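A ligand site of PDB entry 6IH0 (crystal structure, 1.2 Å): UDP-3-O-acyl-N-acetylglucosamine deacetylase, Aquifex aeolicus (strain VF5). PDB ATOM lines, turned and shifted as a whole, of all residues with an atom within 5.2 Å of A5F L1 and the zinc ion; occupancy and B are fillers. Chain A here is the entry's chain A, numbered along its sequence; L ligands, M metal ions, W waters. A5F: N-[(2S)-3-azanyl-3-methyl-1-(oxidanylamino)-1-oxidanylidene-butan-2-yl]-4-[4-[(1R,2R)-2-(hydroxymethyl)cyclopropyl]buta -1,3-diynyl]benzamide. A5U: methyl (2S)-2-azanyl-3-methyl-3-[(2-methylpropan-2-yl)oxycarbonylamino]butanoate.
N5 of A5F L1 is in hydrogen-bond range of OG1 of Thr 179 (3.0 Å). O of His 58 lies within hydrogen-bond range of N7 of A5F L1, at 3.4 Å. A nitrogen (N7) of A5F L1 sits at hydrogen-bond distance from a ring nitrogen (NE2) of His 253. An oxygen (O3) of A5F L1 is in hydrogen-bond range of a ring nitrogen (ND1) of His 58 (3.2 Å). OE2 of Glu 73 sits at hydrogen-bond distance from N7 of A5F L1 (3.1 Å).
NE2 of His 19 lies within hydrogen-bond range of O of His 58, at 3.1 Å. OE2 of Glu 73 lies within hydrogen-bond range of NE2 of His 253 (3.4 Å). N of Thr 179 lies within hydrogen-bond range of ND1 of His 226 (3.3 Å). N of Gly 198 is in hydrogen-bond range of O of Ile 18 (3.4 Å).
Ile 18 touches A5F L1 (CG1 to C27, 3.9 Å). O of Phe 180 touches C17 of A5F L1, 3.5 Å away. Ala 181 touches A5F L1. Ile 189 touches A5F L1. Gly 198 touches A5F L1. Ser 199 touches A5F L1. Leu 200 touches A5F L1 (CD2 to C11, 3.9 Å). OG1 of Thr 203 touches C27 of A5F L1 (3.5 Å). Lys 227 touches A5F L1. Hydrophobic or aromatic side chains that line A5F L1: Ile 18, His 58, His 74, Phe 180, Ala 181, Ile 189, Leu 200, His 226 and His 253. 16 residues have an atom within 4 Å of A5F L1: Ile 18, His 58, Glu 73, His 74, Thr 179, Phe 180, Ala 181, Ile 189, Gly 198, Ser 199, Leu 200, Thr 203, His 226, Lys 227, Asp 230 and His 253.
Three residues have an atom within 4 Å of the zinc ion: His 74, His 226 and Asp 230.
The zinc ion is bound by OD1 of Asp 230, 2.0 Å away. O2 of A5F L1 binds the zinc ion, 2.1 Å away. A ring nitrogen (NE2) of His 74 binds the zinc ion. NE2 of His 226 is bound to the zinc ion. The zinc ion is bound by O04 of A5F L1. Slightly farther from the zinc ion lies OD2 of Asp 230 (2.8 Å).
Water W6 bridges O of Phe 180 and N6 of A5F L1. Water W4 bridges ND1 of His 58 (2.6 Å) and N6 of A5F L1 (3.1 Å). Water W3 lies within hydrogen-bond range of O of His 58 (2.8 Å), OE2 of Glu 73 (2.9 Å), N7 of A5F L1 (3.1 Å) and NE2 of His 19 (3.2 Å). Water W1 lies within hydrogen-bond range of O4 of A5U L2 (2.5 Å), N6 of A5F L1 (3.1 Å) and NZ of Lys 227 (3.2 Å). Water W5 bridges OD2 of Asp 230 (2.9 Å) and NZ of Lys 227 (3.0 Å).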
ATOM      1  N   ILE A  18       9.322  -8.012   0.368  1.00  0.00           N
ATOM      2  CA  ILE A  18       9.660  -7.113   1.471  1.00  0.00           C
ATOM      3  C   ILE A  18      10.868  -7.598   2.264  1.00  0.00           C
ATOM      4  O   ILE A  18      11.671  -6.791   2.757  1.00  0.00           O
ATOM      5  CB  ILE A  18       8.435  -6.845   2.371  1.00  0.00           C
ATOM      6  CG1 ILE A  18       8.708  -5.666   3.303  1.00  0.00           C
ATOM      7  CG2 ILE A  18       8.092  -8.044   3.215  1.00  0.00           C
ATOM      8  CD1 ILE A  18       8.436  -4.350   2.692  1.00  0.00           C
ATOM      9  N   HIS A  19      11.014  -8.912   2.450  1.00  0.00           N
ATOM     10  CA  HIS A  19      12.078  -9.449   3.279  1.00  0.00           C
ATOM     11  C   HIS A  19      13.326  -9.834   2.507  1.00  0.00           C
ATOM     12  O   HIS A  19      14.441  -9.547   2.964  1.00  0.00           O
ATOM     13  CB  HIS A  19      11.594 -10.613   4.134  1.00  0.00           C
ATOM     14  CG  HIS A  19      10.651 -10.165   5.191  1.00  0.00           C
ATOM     15  ND1 HIS A  19      10.970  -9.147   6.061  1.00  0.00           N
ATOM     16  CD2 HIS A  19       9.379 -10.529   5.476  1.00  0.00           C
ATOM     17  CE1 HIS A  19       9.943  -8.925   6.861  1.00  0.00           C
ATOM     18  NE2 HIS A  19       8.963  -9.752   6.525  1.00  0.00           N
ATOM     19  N   HIS A  58       8.055 -12.185  11.622  1.00  0.00           N
ATOM     20  CA  HIS A  58       7.912 -11.054  10.701  1.00  0.00           C
ATOM     21  C   HIS A  58       7.205 -11.411   9.403  1.00  0.00           C
ATOM     22  O   HIS A  58       6.879 -10.501   8.628  1.00  0.00           O
ATOM     23  CB  HIS A  58       9.221 -10.306  10.400  1.00  0.00           C
ATOM     24  CG  HIS A  58       9.881  -9.755  11.624  1.00  0.00           C
ATOM     25  ND1 HIS A  58       9.503  -8.568  12.207  1.00  0.00           N
ATOM     26  CD2 HIS A  58      10.856 -10.270  12.408  1.00  0.00           C
ATOM     27  CE1 HIS A  58      10.249  -8.358  13.279  1.00  0.00           C
ATOM     28  NE2 HIS A  58      11.079  -9.374  13.423  1.00  0.00           N
ATOM     29  N   SER A  59       6.964 -12.678   9.125  1.00  0.00           N
ATOM     30  CA  SER A  59       6.135 -13.107   8.004  1.00  0.00           C
ATOM     31  C   SER A  59       5.753 -14.556   8.287  1.00  0.00           C
ATOM     32  O   SER A  59       6.303 -15.195   9.180  1.00  0.00           O
ATOM     33  CB  SER A  59       6.890 -13.000   6.680  1.00  0.00           C
ATOM     34  OG  SER A  59       8.046 -13.847   6.673  1.00  0.00           O
ATOM     35  N   GLU A  73       1.132 -14.341   3.759  1.00  0.00           N
ATOM     36  CA  GLU A  73      -0.048 -13.935   4.515  1.00  0.00           C
ATOM     37  C   GLU A  73      -0.940 -12.944   3.766  1.00  0.00           C
ATOM     38  O   GLU A  73      -2.158 -12.961   3.938  1.00  0.00           O
ATOM     39  CB  GLU A  73       0.349 -13.395   5.876  1.00  0.00           C
ATOM     40  CG  GLU A  73       1.292 -12.179   5.836  1.00  0.00           C
ATOM     41  CD  GLU A  73       2.773 -12.536   5.928  1.00  0.00           C
ATOM     42  OE1 GLU A  73       3.165 -13.676   5.572  1.00  0.00           O
ATOM     43  OE2 GLU A  73       3.572 -11.668   6.340  1.00  0.00           O
ATOM     44  N   HIS A  74      -0.361 -12.054   2.949  1.00  0.00           N
ATOM     45  CA  HIS A  74      -1.174 -11.009   2.330  1.00  0.00           C
ATOM     46  C   HIS A  74      -1.977 -11.565   1.159  1.00  0.00           C
ATOM     47  O   HIS A  74      -3.185 -11.288   1.051  1.00  0.00           O
ATOM     48  CB  HIS A  74      -0.319  -9.815   1.918  1.00  0.00           C
ATOM     49  CG  HIS A  74       0.498  -9.260   3.045  1.00  0.00           C
ATOM     50  ND1 HIS A  74       1.836  -8.960   2.917  1.00  0.00           N
ATOM     51  CD2 HIS A  74       0.196  -9.027   4.347  1.00  0.00           C
ATOM     52  CE1 HIS A  74       2.306  -8.515   4.075  1.00  0.00           C
ATOM     53  NE2 HIS A  74       1.317  -8.520   4.948  1.00  0.00           N
ATOM     54  N   THR A 179       1.500  -2.822   5.574  1.00  0.00           N
ATOM     55  CA  THR A 179       2.462  -3.250   6.554  1.00  0.00           C
ATOM     56  C   THR A 179       3.213  -2.031   7.110  1.00  0.00           C
ATOM     57  O   THR A 179       3.251  -0.964   6.498  1.00  0.00           O
ATOM     58  CB  THR A 179       3.418  -4.268   5.942  1.00  0.00           C
ATOM     59  OG1 THR A 179       4.134  -4.934   6.988  1.00  0.00           O
ATOM     60  CG2 THR A 179       4.396  -3.633   4.974  1.00  0.00           C
ATOM     61  N   PHE A 180       3.813  -2.211   8.279  1.00  0.00           N
ATOM     62  CA  PHE A 180       4.381  -1.100   9.011  1.00  0.00           C
ATOM     63  C   PHE A 180       5.597  -1.569   9.787  1.00  0.00           C
ATOM     64  O   PHE A 180       5.788  -2.769  10.027  1.00  0.00           O
ATOM     65  CB  PHE A 180       3.341  -0.437   9.932  1.00  0.00           C
ATOM     66  CG  PHE A 180       2.778  -1.366  10.970  1.00  0.00           C
ATOM     67  CD1 PHE A 180       1.703  -2.186  10.679  1.00  0.00           C
ATOM     68  CD2 PHE A 180       3.330  -1.414  12.244  1.00  0.00           C
ATOM     69  CE1 PHE A 180       1.177  -3.039  11.646  1.00  0.00           C
ATOM     70  CE2 PHE A 180       2.813  -2.279  13.203  1.00  0.00           C
ATOM     71  CZ  PHE A 180       1.725  -3.083  12.898  1.00  0.00           C
ATOM     72  N   ALA A 181       6.421  -0.599  10.186  1.00  0.00           N
ATOM     73  CA  ALA A 181       7.629  -0.865  10.945  1.00  0.00           C
ATOM     74  C   ALA A 181       7.973   0.367  11.756  1.00  0.00           C
ATOM     75  O   ALA A 181       7.615   1.492  11.405  1.00  0.00           O
ATOM     76  CB  ALA A 181       8.805  -1.232  10.040  1.00  0.00           C
ATOM     77  N   ILE A 186      14.115  -1.294  13.092  1.00  0.00           N
ATOM     78  CA  ILE A 186      14.484  -1.694  11.735  1.00  0.00           C
ATOM     79  C   ILE A 186      15.909  -2.230  11.689  1.00  0.00           C
ATOM     80  O   ILE A 186      16.196  -3.186  10.955  1.00  0.00           O
ATOM     81  CB  ILE A 186      14.208  -0.564  10.738  1.00  0.00           C
ATOM     82  CG1 ILE A 186      12.699  -0.430  10.495  1.00  0.00           C
ATOM     83  CG2 ILE A 186      14.943  -0.811   9.418  1.00  0.00           C
ATOM     84  CD1 ILE A 186      12.297   0.815   9.746  1.00  0.00           C
ATOM     85  N   ILE A 189      15.821  -5.833  12.642  1.00  0.00           N
ATOM     86  CA  ILE A 189      15.157  -6.631  11.609  1.00  0.00           C
ATOM     87  C   ILE A 189      16.110  -6.899  10.454  1.00  0.00           C
ATOM     88  O   ILE A 189      16.205  -8.031   9.949  1.00  0.00           O
ATOM     89  CB  ILE A 189      13.855  -5.948  11.160  1.00  0.00           C
ATOM     90  CG1 ILE A 189      12.846  -5.928  12.303  1.00  0.00           C
ATOM     91  CG2 ILE A 189      13.282  -6.646   9.946  1.00  0.00           C
ATOM     92  CD1 ILE A 189      11.665  -4.988  12.097  1.00  0.00           C
ATOM     93  N   LYS A 190      16.856  -5.873  10.025  1.00  0.00           N
ATOM     94  CA  LYS A 190      17.822  -6.090   8.969  1.00  0.00           C
ATOM     95  C   LYS A 190      18.960  -6.993   9.423  1.00  0.00           C
ATOM     96  O   LYS A 190      19.424  -7.858   8.668  1.00  0.00           O
ATOM     97  CB  LYS A 190      18.332  -4.744   8.445  1.00  0.00           C
ATOM     98  CG  LYS A 190      17.246  -3.961   7.713  1.00  0.00           C
ATOM     99  CD  LYS A 190      17.775  -2.681   7.102  1.00  0.00           C
ATOM    100  CE  LYS A 190      16.682  -1.956   6.314  1.00  0.00           C
ATOM    101  NZ  LYS A 190      16.424  -2.602   4.986  1.00  0.00           N
ATOM    102  N   GLY A 195      13.591  -7.740   6.044  1.00  0.00           N
ATOM    103  CA  GLY A 195      13.322  -6.356   5.665  1.00  0.00           C
ATOM    104  C   GLY A 195      14.145  -5.801   4.534  1.00  0.00           C
ATOM    105  O   GLY A 195      14.185  -4.576   4.358  1.00  0.00           O
ATOM    106  N   GLY A 198      12.217  -3.437   2.234  1.00  0.00           N
ATOM    107  CA  GLY A 198      11.381  -2.413   2.838  1.00  0.00           C
ATOM    108  C   GLY A 198      11.797  -1.016   2.440  1.00  0.00           C
ATOM    109  O   GLY A 198      12.984  -0.697   2.381  1.00  0.00           O
ATOM    110  N   SER A 199      10.805  -0.169   2.192  1.00  0.00           N
ATOM    111  CA  SER A 199      11.066   1.220   1.839  1.00  0.00           C
ATOM    112  C   SER A 199       9.793   2.004   2.126  1.00  0.00           C
ATOM    113  O   SER A 199       8.743   1.433   2.431  1.00  0.00           O
ATOM    114  CB  SER A 199      11.422   1.368   0.361  1.00  0.00           C
ATOM    115  OG  SER A 199      10.251   1.252  -0.425  1.00  0.00           O
ATOM    116  N   LEU A 200       9.888   3.318   1.989  1.00  0.00           N
ATOM    117  CA  LEU A 200       8.696   4.147   2.155  1.00  0.00           C
ATOM    118  C   LEU A 200       7.699   3.946   1.033  1.00  0.00           C
ATOM    119  O   LEU A 200       6.577   4.459   1.136  1.00  0.00           O
ATOM    120  CB  LEU A 200       9.090   5.611   2.278  1.00  0.00           C
ATOM    121  CG  LEU A 200       9.984   5.962   3.476  1.00  0.00           C
ATOM    122  CD1 LEU A 200      10.286   7.453   3.467  1.00  0.00           C
ATOM    123  CD2 LEU A 200       9.325   5.551   4.772  1.00  0.00           C
ATOM    124  N   THR A 203       6.020   0.381   2.903  1.00  0.00           N
ATOM    125  CA  THR A 203       5.914   0.198   4.345  1.00  0.00           C
ATOM    126  C   THR A 203       5.588   1.546   4.966  1.00  0.00           C
ATOM    127  O   THR A 203       6.172   2.569   4.604  1.00  0.00           O
ATOM    128  CB  THR A 203       7.251  -0.289   4.919  1.00  0.00           C
ATOM    129  OG1 THR A 203       7.630  -1.505   4.271  1.00  0.00           O
ATOM    130  CG2 THR A 203       7.163  -0.530   6.407  1.00  0.00           C
ATOM    131  N   VAL A 205       6.362   3.649   7.867  1.00  0.00           N
ATOM    132  CA  VAL A 205       7.476   3.688   8.800  1.00  0.00           C
ATOM    133  C   VAL A 205       7.221   4.773   9.828  1.00  0.00           C
ATOM    134  O   VAL A 205       7.042   5.940   9.470  1.00  0.00           O
ATOM    135  CB  VAL A 205       8.829   3.870   8.084  1.00  0.00           C
ATOM    136  CG1 VAL A 205       9.946   3.925   9.107  1.00  0.00           C
ATOM    137  CG2 VAL A 205       9.054   2.725   7.110  1.00  0.00           C
ATOM    138  N   TYR A 212       7.299   8.786   8.890  1.00  0.00           N
ATOM    139  CA  TYR A 212       8.320   9.034   7.875  1.00  0.00           C
ATOM    140  C   TYR A 212       7.717   9.234   6.489  1.00  0.00           C
ATOM    141  O   TYR A 212       8.220  10.042   5.697  1.00  0.00           O
ATOM    142  CB  TYR A 212       9.341   7.902   7.857  1.00  0.00           C
ATOM    143  CG  TYR A 212      10.333   7.926   8.981  1.00  0.00           C
ATOM    144  CD1 TYR A 212       9.974   7.554  10.264  1.00  0.00           C
ATOM    145  CD2 TYR A 212      11.656   8.314   8.766  1.00  0.00           C
ATOM    146  CE1 TYR A 212      10.884   7.569  11.308  1.00  0.00           C
ATOM    147  CE2 TYR A 212      12.584   8.327   9.797  1.00  0.00           C
ATOM    148  CZ  TYR A 212      12.192   7.958  11.063  1.00  0.00           C
ATOM    149  OH  TYR A 212      13.099   7.979  12.095  1.00  0.00           O
ATOM    150  N   HIS A 226      -4.065  -3.465   9.480  1.00  0.00           N
ATOM    151  CA  HIS A 226      -3.148  -4.393   8.825  1.00  0.00           C
ATOM    152  C   HIS A 226      -2.990  -5.674   9.622  1.00  0.00           C
ATOM    153  O   HIS A 226      -2.908  -6.766   9.043  1.00  0.00           O
ATOM    154  CB  HIS A 226      -1.788  -3.753   8.571  1.00  0.00           C
ATOM    155  CG  HIS A 226      -0.916  -4.646   7.764  1.00  0.00           C
ATOM    156  ND1 HIS A 226      -1.043  -4.740   6.397  1.00  0.00           N
ATOM    157  CD2 HIS A 226      -0.024  -5.591   8.130  1.00  0.00           C
ATOM    158  CE1 HIS A 226      -0.216  -5.678   5.948  1.00  0.00           C
ATOM    159  NE2 HIS A 226       0.403  -6.209   6.979  1.00  0.00           N
ATOM    160  N   LYS A 227      -2.920  -5.586  10.946  1.00  0.00           N
ATOM    161  CA  LYS A 227      -2.791  -6.789  11.765  1.00  0.00           C
ATOM    162  C   LYS A 227      -4.020  -7.686  11.645  1.00  0.00           C
ATOM    163  O   LYS A 227      -3.889  -8.919  11.682  1.00  0.00           O
ATOM    164  CB  LYS A 227      -2.496  -6.429  13.216  1.00  0.00           C
ATOM    165  CG  LYS A 227      -1.159  -5.732  13.412  1.00  0.00           C
ATOM    166  CD  LYS A 227       0.012  -6.684  13.222  1.00  0.00           C
ATOM    167  CE  LYS A 227       0.127  -7.652  14.384  1.00  0.00           C
ATOM    168  NZ  LYS A 227       1.430  -8.366  14.441  1.00  0.00           N
ATOM    169  N   ASP A 230      -3.519  -9.436   8.346  1.00  0.00           N
ATOM    170  CA  ASP A 230      -2.552 -10.528   8.514  1.00  0.00           C
ATOM    171  C   ASP A 230      -3.213 -11.755   9.128  1.00  0.00           C
ATOM    172  O   ASP A 230      -2.964 -12.896   8.698  1.00  0.00           O
ATOM    173  CB  ASP A 230      -1.417 -10.099   9.453  1.00  0.00           C
ATOM    174  CG  ASP A 230      -0.358  -9.233   8.794  1.00  0.00           C
ATOM    175  OD1 ASP A 230      -0.247  -9.159   7.553  1.00  0.00           O
ATOM    176  OD2 ASP A 230       0.405  -8.624   9.585  1.00  0.00           O
ATOM    177  N   HIS A 253       2.283 -13.402  13.824  1.00  0.00           N
ATOM    178  CA  HIS A 253       2.175 -14.633  13.030  1.00  0.00           C
ATOM    179  C   HIS A 253       2.400 -15.886  13.871  1.00  0.00           C
ATOM    180  O   HIS A 253       1.734 -16.899  13.641  1.00  0.00           O
ATOM    181  CB  HIS A 253       3.149 -14.641  11.867  1.00  0.00           C
ATOM    182  CG  HIS A 253       2.965 -13.482  10.943  1.00  0.00           C
ATOM    183  ND1 HIS A 253       1.798 -13.259  10.244  1.00  0.00           N
ATOM    184  CD2 HIS A 253       3.809 -12.471  10.620  1.00  0.00           C
ATOM    185  CE1 HIS A 253       1.941 -12.152   9.530  1.00  0.00           C
ATOM    186  NE2 HIS A 253       3.145 -11.658   9.743  1.00  0.00           N
HETATM  187  C10 A5F L   1      14.311   2.307   6.269  1.00  0.00           C
HETATM  188  C8  A5F L   1      12.949   2.970   6.088  1.00  0.00           C
HETATM  189  C9  A5F L   1      13.325   1.765   5.227  1.00  0.00           C
HETATM  190  C11 A5F L   1      12.939   4.319   5.345  1.00  0.00           C
HETATM  191  C12 A5F L   1      12.612   0.473   5.626  1.00  0.00           C
HETATM  192  C13 A5F L   1       4.159  -6.912  10.799  1.00  0.00           C
HETATM  193  C14 A5F L   1       4.792  -7.547   9.537  1.00  0.00           C
HETATM  194  C15 A5F L   1      12.039  -0.513   5.934  1.00  0.00           C
HETATM  195  C16 A5F L   1       2.969  -7.781  11.266  1.00  0.00           C
HETATM  196  C17 A5F L   1       3.652  -5.474  10.522  1.00  0.00           C
HETATM  197  C18 A5F L   1       3.729  -7.954   8.550  1.00  0.00           C
HETATM  198  C19 A5F L   1       7.100  -6.783   9.149  1.00  0.00           C
HETATM  199  C20 A5F L   1      11.268  -1.751   6.357  1.00  0.00           C
HETATM  200  C21 A5F L   1       7.949  -5.760   8.474  1.00  0.00           C
HETATM  201  C22 A5F L   1       9.306  -5.549   9.109  1.00  0.00           C
HETATM  202  C23 A5F L   1       7.414  -4.924   7.318  1.00  0.00           C
HETATM  203  C24 A5F L   1       9.683  -3.672   7.358  1.00  0.00           C
HETATM  204  C25 A5F L   1      10.588  -2.604   6.787  1.00  0.00           C
HETATM  205  C26 A5F L   1      10.200  -4.484   8.530  1.00  0.00           C
HETATM  206  C27 A5F L   1       8.308  -3.858   6.740  1.00  0.00           C
HETATM  207  N5  A5F L   1       5.691  -6.644   8.901  1.00  0.00           N
HETATM  208  N6  A5F L   1       5.171  -6.820  11.868  1.00  0.00           N
HETATM  209  N7  A5F L   1       3.641  -9.355   8.384  1.00  0.00           N
HETATM  210  O1  A5F L   1      13.192   5.366   6.257  1.00  0.00           O
HETATM  211  O2  A5F L   1       3.014  -7.219   7.915  1.00  0.00           O
HETATM  212  O3  A5F L   1       7.528  -7.552   9.952  1.00  0.00           O
HETATM  213  O04 A5F L   1       2.642  -9.722   7.481  1.00  0.00           O
HETATM  214  C10 A5U L   2       7.012 -10.084  17.511  1.00  0.00           C
HETATM  215  C11 A5U L   2       4.983 -10.611  13.451  1.00  0.00           C
HETATM  216  C12 A5U L   2       9.591  -8.521  17.970  1.00  0.00           C
HETATM  217  C13 A5U L   2       5.630  -9.296  15.186  1.00  0.00           C
HETATM  218  C14 A5U L   2       3.474 -10.636  13.310  1.00  0.00           C
HETATM  219  C15 A5U L   2       5.591  -9.638  12.447  1.00  0.00           C
HETATM  220  C16 A5U L   2       5.591 -11.965  13.276  1.00  0.00           C
HETATM  221  C17 A5U L   2       9.408  -6.593  19.366  1.00  0.00           C
HETATM  222  C7  A5U L   2       7.609  -9.017  16.584  1.00  0.00           C
HETATM  223  C8  A5U L   2       9.154  -9.072  16.618  1.00  0.00           C
HETATM  224  C9  A5U L   2       7.151  -7.630  17.013  1.00  0.00           C
HETATM  225  N5  A5U L   2       7.095  -9.203  15.250  1.00  0.00           N
HETATM  226  N6  A5U L   2       9.616 -10.425  16.485  1.00  0.00           N
HETATM  227  O1  A5U L   2       5.154 -10.519  14.833  1.00  0.00           O
HETATM  228  O2  A5U L   2       9.885  -7.141  18.154  1.00  0.00           O
HETATM  229  O3  A5U L   2       9.681  -9.260  18.887  1.00  0.00           O
HETATM  230  O4  A5U L   2       4.843  -8.426  15.428  1.00  0.00           O
HETATM  231 ZN    ZN M   1       1.375  -8.071   6.977  1.00  0.00          ZN
HETATM  232  O   HOH W   1       3.841  -6.256  14.634  1.00  0.00           O
HETATM  233  O   HOH W   2       5.025  -7.273   5.191  1.00  0.00           O
HETATM  234  O   HOH W   3       5.796  -9.763   6.200  1.00  0.00           O
HETATM  235  O   HOH W   4       8.082  -6.478  12.817  1.00  0.00           O
HETATM  236  O   HOH W   5       0.673 -10.037  12.050  1.00  0.00           O
HETATM  237  O   HOH W   6       7.026  -4.444  11.713  1.00  0.00           O
